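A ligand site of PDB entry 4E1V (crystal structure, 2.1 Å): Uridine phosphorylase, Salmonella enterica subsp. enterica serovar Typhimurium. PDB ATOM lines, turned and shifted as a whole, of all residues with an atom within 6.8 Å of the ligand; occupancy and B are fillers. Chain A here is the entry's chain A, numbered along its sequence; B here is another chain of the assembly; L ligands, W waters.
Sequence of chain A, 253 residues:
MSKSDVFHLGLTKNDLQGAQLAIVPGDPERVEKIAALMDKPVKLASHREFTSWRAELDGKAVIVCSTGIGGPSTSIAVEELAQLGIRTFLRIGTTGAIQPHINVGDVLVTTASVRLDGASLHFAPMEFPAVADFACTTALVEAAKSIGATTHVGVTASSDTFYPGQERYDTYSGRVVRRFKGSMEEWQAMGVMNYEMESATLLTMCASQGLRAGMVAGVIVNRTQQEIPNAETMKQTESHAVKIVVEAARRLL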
ATOM      1  N   THR A  94       2.130 -18.732 -23.972  1.00  0.00           N
ATOM      2  CA  THR A  94       2.344 -18.809 -25.397  1.00  0.00           C
ATOM      3  C   THR A  94       2.533 -17.397 -25.937  1.00  0.00           C
ATOM      4  O   THR A  94       2.133 -16.422 -25.301  1.00  0.00           O
ATOM      5  CB  THR A  94       1.148 -19.422 -26.117  1.00  0.00           C
ATOM      6  OG1 THR A  94      -0.010 -18.630 -25.840  1.00  0.00           O
ATOM      7  CG2 THR A  94       0.938 -20.861 -25.660  1.00  0.00           C
ATOM      8  N   THR A  95       3.137 -17.297 -27.112  1.00  0.00           N
ATOM      9  CA  THR A  95       3.458 -16.007 -27.675  1.00  0.00           C
ATOM     10  C   THR A  95       3.553 -16.042 -29.202  1.00  0.00           C
ATOM     11  O   THR A  95       3.720 -17.103 -29.809  1.00  0.00           O
ATOM     12  CB  THR A  95       4.758 -15.456 -27.087  1.00  0.00           C
ATOM     13  OG1 THR A  95       4.887 -14.076 -27.452  1.00  0.00           O
ATOM     14  CG2 THR A  95       5.959 -16.222 -27.600  1.00  0.00           C
ATOM     15  N   GLY A  96       3.394 -14.876 -29.803  1.00  0.00           N
ATOM     16  CA  GLY A  96       3.629 -14.736 -31.219  1.00  0.00           C
ATOM     17  C   GLY A  96       4.854 -13.889 -31.479  1.00  0.00           C
ATOM     18  O   GLY A  96       4.925 -12.751 -31.033  1.00  0.00           O
ATOM     19  N   ALA A  97       5.808 -14.462 -32.221  1.00  0.00           N
ATOM     20  CA  ALA A  97       7.040 -13.778 -32.589  1.00  0.00           C
ATOM     21  C   ALA A  97       6.810 -12.761 -33.691  1.00  0.00           C
ATOM     22  O   ALA A  97       5.957 -12.955 -34.551  1.00  0.00           O
ATOM     23  CB  ALA A  97       8.089 -14.792 -33.031  1.00  0.00           C
ATOM     24  N   ALA A 157       6.924  -7.304 -26.186  1.00  0.00           N
ATOM     25  CA  ALA A 157       5.879  -6.288 -26.186  1.00  0.00           C
ATOM     26  C   ALA A 157       4.608  -6.842 -25.552  1.00  0.00           C
ATOM     27  O   ALA A 157       3.995  -7.785 -26.053  1.00  0.00           O
ATOM     28  CB  ALA A 157       5.594  -5.766 -27.589  1.00  0.00           C
ATOM     29  N   SER A 159       0.855  -6.411 -24.502  1.00  0.00           N
ATOM     30  CA  SER A 159      -0.293  -5.664 -24.984  1.00  0.00           C
ATOM     31  C   SER A 159      -1.596  -5.981 -24.259  1.00  0.00           C
ATOM     32  O   SER A 159      -1.926  -7.143 -24.033  1.00  0.00           O
ATOM     33  CB  SER A 159      -0.485  -5.947 -26.474  1.00  0.00           C
ATOM     34  OG  SER A 159      -1.780  -5.579 -26.882  1.00  0.00           O
ATOM     35  N   THR A 161      -4.550  -5.807 -25.451  1.00  0.00           N
ATOM     36  CA  THR A 161      -5.493  -6.506 -26.341  1.00  0.00           C
ATOM     37  C   THR A 161      -4.755  -7.572 -27.178  1.00  0.00           C
ATOM     38  O   THR A 161      -3.526  -7.528 -27.300  1.00  0.00           O
ATOM     39  CB  THR A 161      -6.215  -5.528 -27.315  1.00  0.00           C
ATOM     40  OG1 THR A 161      -5.245  -4.894 -28.158  1.00  0.00           O
ATOM     41  CG2 THR A 161      -7.031  -4.472 -26.567  1.00  0.00           C
ATOM     42  N   PHE A 162      -5.512  -8.519 -27.743  1.00  0.00           N
ATOM     43  CA  PHE A 162      -4.966  -9.546 -28.651  1.00  0.00           C
ATOM     44  C   PHE A 162      -4.925  -9.004 -30.077  1.00  0.00           C
ATOM     45  O   PHE A 162      -4.007  -9.294 -30.837  1.00  0.00           O
ATOM     46  CB  PHE A 162      -5.813 -10.836 -28.588  1.00  0.00           C
ATOM     47  CG  PHE A 162      -5.271 -12.009 -29.417  1.00  0.00           C
ATOM     48  CD1 PHE A 162      -5.814 -12.315 -30.652  1.00  0.00           C
ATOM     49  CD2 PHE A 162      -4.242 -12.802 -28.930  1.00  0.00           C
ATOM     50  CE1 PHE A 162      -5.333 -13.396 -31.407  1.00  0.00           C
ATOM     51  CE2 PHE A 162      -3.756 -13.875 -29.667  1.00  0.00           C
ATOM     52  CZ  PHE A 162      -4.302 -14.172 -30.906  1.00  0.00           C
ATOM     53  N   GLN A 166      -1.884  -5.698 -30.945  1.00  0.00           N
ATOM     54  CA  GLN A 166      -0.847  -6.479 -31.624  1.00  0.00           C
ATOM     55  C   GLN A 166      -0.973  -6.287 -33.144  1.00  0.00           C
ATOM     56  O   GLN A 166      -0.569  -7.146 -33.935  1.00  0.00           O
ATOM     57  CB  GLN A 166      -0.920  -7.961 -31.216  1.00  0.00           C
ATOM     58  CG  GLN A 166      -0.868  -8.165 -29.707  1.00  0.00           C
ATOM     59  CD  GLN A 166      -0.800  -9.627 -29.275  1.00  0.00           C
ATOM     60  OE1 GLN A 166      -0.453 -10.519 -30.059  1.00  0.00           O
ATOM     61  NE2 GLN A 166      -1.120  -9.867 -28.006  1.00  0.00           N
ATOM     62  N   ARG A 168      -3.384  -6.512 -35.405  1.00  0.00           N
ATOM     63  CA  ARG A 168      -4.121  -7.444 -36.251  1.00  0.00           C
ATOM     64  C   ARG A 168      -5.238  -6.690 -36.980  1.00  0.00           C
ATOM     65  O   ARG A 168      -6.011  -5.967 -36.351  1.00  0.00           O
ATOM     66  CB  ARG A 168      -4.712  -8.589 -35.417  1.00  0.00           C
ATOM     67  CG  ARG A 168      -3.682  -9.622 -34.979  1.00  0.00           C
ATOM     68  CD  ARG A 168      -4.274 -10.821 -34.199  1.00  0.00           C
ATOM     69  NE  ARG A 168      -3.346 -11.961 -34.250  1.00  0.00           N
ATOM     70  CZ  ARG A 168      -2.407 -12.209 -33.334  1.00  0.00           C
ATOM     71  NH1 ARG A 168      -1.606 -13.244 -33.492  1.00  0.00           N
ATOM     72  NH2 ARG A 168      -2.273 -11.430 -32.280  1.00  0.00           N
ATOM     73  N   TYR A 195       4.981 -10.739 -29.044  1.00  0.00           N
ATOM     74  CA  TYR A 195       3.843 -10.152 -28.353  1.00  0.00           C
ATOM     75  C   TYR A 195       3.283 -11.148 -27.357  1.00  0.00           C
ATOM     76  O   TYR A 195       3.188 -12.345 -27.658  1.00  0.00           O
ATOM     77  CB  TYR A 195       2.718  -9.842 -29.340  1.00  0.00           C
ATOM     78  CG  TYR A 195       2.826  -8.587 -30.172  1.00  0.00           C
ATOM     79  CD1 TYR A 195       2.780  -7.329 -29.583  1.00  0.00           C
ATOM     80  CD2 TYR A 195       2.870  -8.658 -31.569  1.00  0.00           C
ATOM     81  CE1 TYR A 195       2.842  -6.172 -30.359  1.00  0.00           C
ATOM     82  CE2 TYR A 195       2.934  -7.523 -32.347  1.00  0.00           C
ATOM     83  CZ  TYR A 195       2.913  -6.278 -31.747  1.00  0.00           C
ATOM     84  OH  TYR A 195       2.970  -5.139 -32.513  1.00  0.00           O
ATOM     85  N   GLU A 196       2.919 -10.665 -26.181  1.00  0.00           N
ATOM     86  CA  GLU A 196       1.982 -11.387 -25.329  1.00  0.00           C
ATOM     87  C   GLU A 196       1.141 -10.396 -24.511  1.00  0.00           C
ATOM     88  O   GLU A 196       1.149  -9.197 -24.820  1.00  0.00           O
ATOM     89  CB  GLU A 196       2.679 -12.462 -24.474  1.00  0.00           C
ATOM     90  CG  GLU A 196       3.845 -11.960 -23.685  1.00  0.00           C
ATOM     91  CD  GLU A 196       3.401 -11.146 -22.514  1.00  0.00           C
ATOM     92  OE1 GLU A 196       3.052 -11.736 -21.474  1.00  0.00           O
ATOM     93  OE2 GLU A 196       3.386  -9.900 -22.636  1.00  0.00           O
ATOM     94  N   MET A 197       0.422 -10.863 -23.503  1.00  0.00           N
ATOM     95  CA  MET A 197      -0.549  -9.988 -22.848  1.00  0.00           C
ATOM     96  C   MET A 197      -0.421  -9.821 -21.335  1.00  0.00           C
ATOM     97  O   MET A 197      -1.264  -9.162 -20.716  1.00  0.00           O
ATOM     98  CB  MET A 197      -1.986 -10.406 -23.214  1.00  0.00           C
ATOM     99  CG  MET A 197      -2.261 -10.386 -24.697  1.00  0.00           C
ATOM    100  SD  MET A 197      -3.942 -10.887 -25.134  1.00  0.00           S
ATOM    101  CE  MET A 197      -4.866  -9.682 -24.202  1.00  0.00           C
ATOM    102  N   GLU A 198       0.619 -10.388 -20.728  1.00  0.00           N
ATOM    103  CA  GLU A 198       0.699 -10.392 -19.260  1.00  0.00           C
ATOM    104  C   GLU A 198       1.986  -9.844 -18.645  1.00  0.00           C
ATOM    105  O   GLU A 198       1.961  -9.350 -17.524  1.00  0.00           O
ATOM    106  CB  GLU A 198       0.421 -11.795 -18.701  1.00  0.00           C
ATOM    107  CG  GLU A 198      -1.040 -12.275 -18.853  1.00  0.00           C
ATOM    108  CD  GLU A 198      -1.319 -12.932 -20.209  1.00  0.00           C
ATOM    109  OE1 GLU A 198      -0.364 -13.418 -20.844  1.00  0.00           O
ATOM    110  OE2 GLU A 198      -2.500 -12.972 -20.630  1.00  0.00           O
ATOM    111  N   GLY A 218       6.602 -20.101 -25.135  1.00  0.00           N
ATOM    112  CA  GLY A 218       6.802 -20.885 -26.337  1.00  0.00           C
ATOM    113  C   GLY A 218       6.112 -20.227 -27.500  1.00  0.00           C
ATOM    114  O   GLY A 218       4.946 -19.811 -27.388  1.00  0.00           O
ATOM    115  N   VAL A 219       6.815 -20.105 -28.619  1.00  0.00           N
ATOM    116  CA  VAL A 219       6.247 -19.458 -29.795  1.00  0.00           C
ATOM    117  C   VAL A 219       5.249 -20.380 -30.492  1.00  0.00           C
ATOM    118  O   VAL A 219       5.558 -21.539 -30.764  1.00  0.00           O
ATOM    119  CB  VAL A 219       7.358 -19.071 -30.786  1.00  0.00           C
ATOM    120  CG1 VAL A 219       6.772 -18.509 -32.055  1.00  0.00           C
ATOM    121  CG2 VAL A 219       8.335 -18.085 -30.136  1.00  0.00           C
ATOM    122  N   ILE A 220       4.053 -19.882 -30.770  1.00  0.00           N
ATOM    123  CA  ILE A 220       3.042 -20.695 -31.434  1.00  0.00           C
ATOM    124  C   ILE A 220       2.636 -20.119 -32.799  1.00  0.00           C
ATOM    125  O   ILE A 220       1.772 -20.671 -33.472  1.00  0.00           O
ATOM    126  CB  ILE A 220       1.777 -20.870 -30.569  1.00  0.00           C
ATOM    127  CG1 ILE A 220       1.008 -19.555 -30.445  1.00  0.00           C
ATOM    128  CG2 ILE A 220       2.154 -21.449 -29.196  1.00  0.00           C
ATOM    129  CD1 ILE A 220      -0.309 -19.694 -29.707  1.00  0.00           C
ATOM    130  N   VAL A 221       3.254 -19.003 -33.166  1.00  0.00           N
ATOM    131  CA  VAL A 221       3.039 -18.396 -34.479  1.00  0.00           C
ATOM    132  C   VAL A 221       4.103 -17.347 -34.746  1.00  0.00           C
ATOM    133  O   VAL A 221       4.605 -16.720 -33.815  1.00  0.00           O
ATOM    134  CB  VAL A 221       1.662 -17.707 -34.586  1.00  0.00           C
ATOM    135  CG1 VAL A 221       1.671 -16.415 -33.800  1.00  0.00           C
ATOM    136  CG2 VAL A 221       1.341 -17.418 -36.055  1.00  0.00           C
ATOM    137  N   ARG A 223       4.488 -13.826 -36.707  1.00  0.00           N
ATOM    138  CA  ARG A 223       3.670 -12.777 -37.307  1.00  0.00           C
ATOM    139  C   ARG A 223       4.166 -12.280 -38.667  1.00  0.00           C
ATOM    140  O   ARG A 223       3.392 -11.705 -39.434  1.00  0.00           O
ATOM    141  CB  ARG A 223       3.466 -11.612 -36.332  1.00  0.00           C
ATOM    142  CG  ARG A 223       2.603 -11.957 -35.129  1.00  0.00           C
ATOM    143  CD  ARG A 223       1.159 -12.164 -35.544  1.00  0.00           C
ATOM    144  NE  ARG A 223       0.678 -10.990 -36.272  1.00  0.00           N
ATOM    145  CZ  ARG A 223       0.204  -9.891 -35.696  1.00  0.00           C
ATOM    146  NH1 ARG A 223       0.129  -9.821 -34.370  1.00  0.00           N
ATOM    147  NH2 ARG A 223      -0.191  -8.866 -36.434  1.00  0.00           N
ATOM    148  N   GLU A 227      -1.351 -14.095 -39.191  1.00  0.00           N
ATOM    149  CA  GLU A 227      -1.977 -13.458 -38.030  1.00  0.00           C
ATOM    150  C   GLU A 227      -2.400 -14.461 -36.963  1.00  0.00           C
ATOM    151  O   GLU A 227      -2.110 -14.277 -35.779  1.00  0.00           O
ATOM    152  CB  GLU A 227      -3.187 -12.606 -38.431  1.00  0.00           C
ATOM    153  CG  GLU A 227      -2.860 -11.145 -38.735  1.00  0.00           C
ATOM    154  CD  GLU A 227      -4.084 -10.224 -38.703  1.00  0.00           C
ATOM    155  OE1 GLU A 227      -3.991  -9.114 -39.286  1.00  0.00           O
ATOM    156  OE2 GLU A 227      -5.125 -10.598 -38.107  1.00  0.00           O
ATOM    157  N   PRO A 229      -2.396 -18.324 -35.338  1.00  0.00           N
ATOM    158  CA  PRO A 229      -1.636 -19.571 -35.287  1.00  0.00           C
ATOM    159  C   PRO A 229      -2.450 -20.735 -35.841  1.00  0.00           C
ATOM    160  O   PRO A 229      -3.668 -20.770 -35.647  1.00  0.00           O
ATOM    161  CB  PRO A 229      -1.389 -19.766 -33.786  1.00  0.00           C
ATOM    162  CG  PRO A 229      -1.548 -18.411 -33.189  1.00  0.00           C
ATOM    163  CD  PRO A 229      -2.616 -17.755 -33.999  1.00  0.00           C
ATOM    164  N   PHE B   7     -10.403 -17.624 -32.726  1.00  0.00           N
ATOM    165  CA  PHE B   7      -9.264 -18.228 -32.047  1.00  0.00           C
ATOM    166  C   PHE B   7      -9.460 -18.567 -30.573  1.00  0.00           C
ATOM    167  O   PHE B   7      -9.027 -19.629 -30.143  1.00  0.00           O
ATOM    168  CB  PHE B   7      -7.997 -17.394 -32.278  1.00  0.00           C
ATOM    169  CG  PHE B   7      -6.752 -18.045 -31.751  1.00  0.00           C
ATOM    170  CD1 PHE B   7      -6.183 -19.116 -32.419  1.00  0.00           C
ATOM    171  CD2 PHE B   7      -6.144 -17.592 -30.598  1.00  0.00           C
ATOM    172  CE1 PHE B   7      -5.032 -19.722 -31.946  1.00  0.00           C
ATOM    173  CE2 PHE B   7      -4.993 -18.185 -30.120  1.00  0.00           C
ATOM    174  CZ  PHE B   7      -4.433 -19.257 -30.786  1.00  0.00           C
ATOM    175  N   HIS B   8     -10.107 -17.710 -29.788  1.00  0.00           N
ATOM    176  CA  HIS B   8     -10.258 -18.002 -28.358  1.00  0.00           C
ATOM    177  C   HIS B   8     -11.553 -18.698 -27.958  1.00  0.00           C
ATOM    178  O   HIS B   8     -11.552 -19.598 -27.122  1.00  0.00           O
ATOM    179  CB  HIS B   8     -10.053 -16.753 -27.489  1.00  0.00           C
ATOM    180  CG  HIS B   8      -8.690 -16.155 -27.625  1.00  0.00           C
ATOM    181  ND1 HIS B   8      -8.319 -15.389 -28.706  1.00  0.00           N
ATOM    182  CD2 HIS B   8      -7.605 -16.242 -26.830  1.00  0.00           C
ATOM    183  CE1 HIS B   8      -7.056 -15.020 -28.556  1.00  0.00           C
ATOM    184  NE2 HIS B   8      -6.604 -15.516 -27.430  1.00  0.00           N
HETATM  185  N1  LIG L   1      -0.400 -14.661 -27.419  1.00  0.00           N
HETATM  186  C1  LIG L   1      -0.463 -13.291 -27.867  1.00  0.00           C
HETATM  187  N2  LIG L   1      -0.252 -12.995 -29.235  1.00  0.00           N
HETATM  188  C2  LIG L   1       0.030 -14.018 -30.147  1.00  0.00           C
HETATM  189  C3  LIG L   1       0.112 -15.419 -29.678  1.00  0.00           C
HETATM  190  C4  LIG L   1      -0.102 -15.726 -28.361  1.00  0.00           C
HETATM  191  O1  LIG L   1      -0.709 -12.401 -27.061  1.00  0.00           O
HETATM  192  O2  LIG L   1       0.214 -13.742 -31.330  1.00  0.00           O
HETATM  193  F1  LIG L   1       0.370 -16.385 -30.542  1.00  0.00           F
HETATM  194  O   HOH W   1       1.368 -11.333 -32.348  1.00  0.00           O
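The backbone NH (N) of Gly 96 sits close to a fluorine (F1) of the ligand, 3.5 Å away. Merely in contact with the ligand: Ile 220 (3.2 Å), Glu 196 (3.4 Å), Thr 95 (3.5 Å), Met 197 (3.5 Å), Val 221 (3.5 Å), Phe 162 (3.6 Å), Thr 94 (3.7 Å), Tyr 195 (3.8 Å) and Pro 229 (3.8 Å). Hydrophobic or aromatic side chains that line the ligand: Phe 162, Met 197, Ile 220, Val 221 and Pro 229. 12 residues have an atom within 4 Å of the ligand: Thr 94, Thr 95, Gly 96, Phe 162, Gln 166, Arg 168, Tyr 195, Glu 196, Met 197, Ile 220, Val 221 and Pro 229. The nearest printed residue that does not touch the ligand is Arg 223 (4.6 Å).
Water W1 lies within hydrogen-bond range of the guanidinium group (NH1) of Arg 223 (2.8 Å), an oxygen (O2) of the ligand (2.9 Å) and the side-chain amide oxygen (OE1) of Gln 166 (3.0 Å).
OE1 of Gln 166 lies within hydrogen-bond range of N2 of the ligand, 2.6 Å away. An oxygen (O2) of the ligand lies within hydrogen-bond range of the guanidinium group (NH1) of Arg 168, at 2.9 Å.
The backbone carbonyl oxygen of Glu 227 is in hydrogen-bond range of the guanidinium group of Arg 168, at 2.6 Å. The backbone carbonyl oxygen of Gly 218 is in hydrogen-bond range of the backbone NH of Thr 95, 3.1 Å away. The backbone carbonyl oxygen (O) of Gly 96 lies within hydrogen-bond range of the backbone NH (N) of Tyr 195, 2.8 Å away. The side-chain amide oxygen (OE1) of Gln 166 is in hydrogen-bond range of the guanidinium group (NH2) of Arg 168, at 3.0 Å. The backbone carbonyl oxygen of Glu 196 is in hydrogen-bond range of the backbone NH of Ser 159. The backbone NH of Glu 196 sits at hydrogen-bond distance from the backbone carbonyl oxygen of Ala 157, 3.1 Å away. OE1 of Glu 196 sits at hydrogen-bond distance from N of Glu 198 (2.9 Å). OG1 of Thr 95 is in hydrogen-bond range of O of Tyr 195 (2.4 Å).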
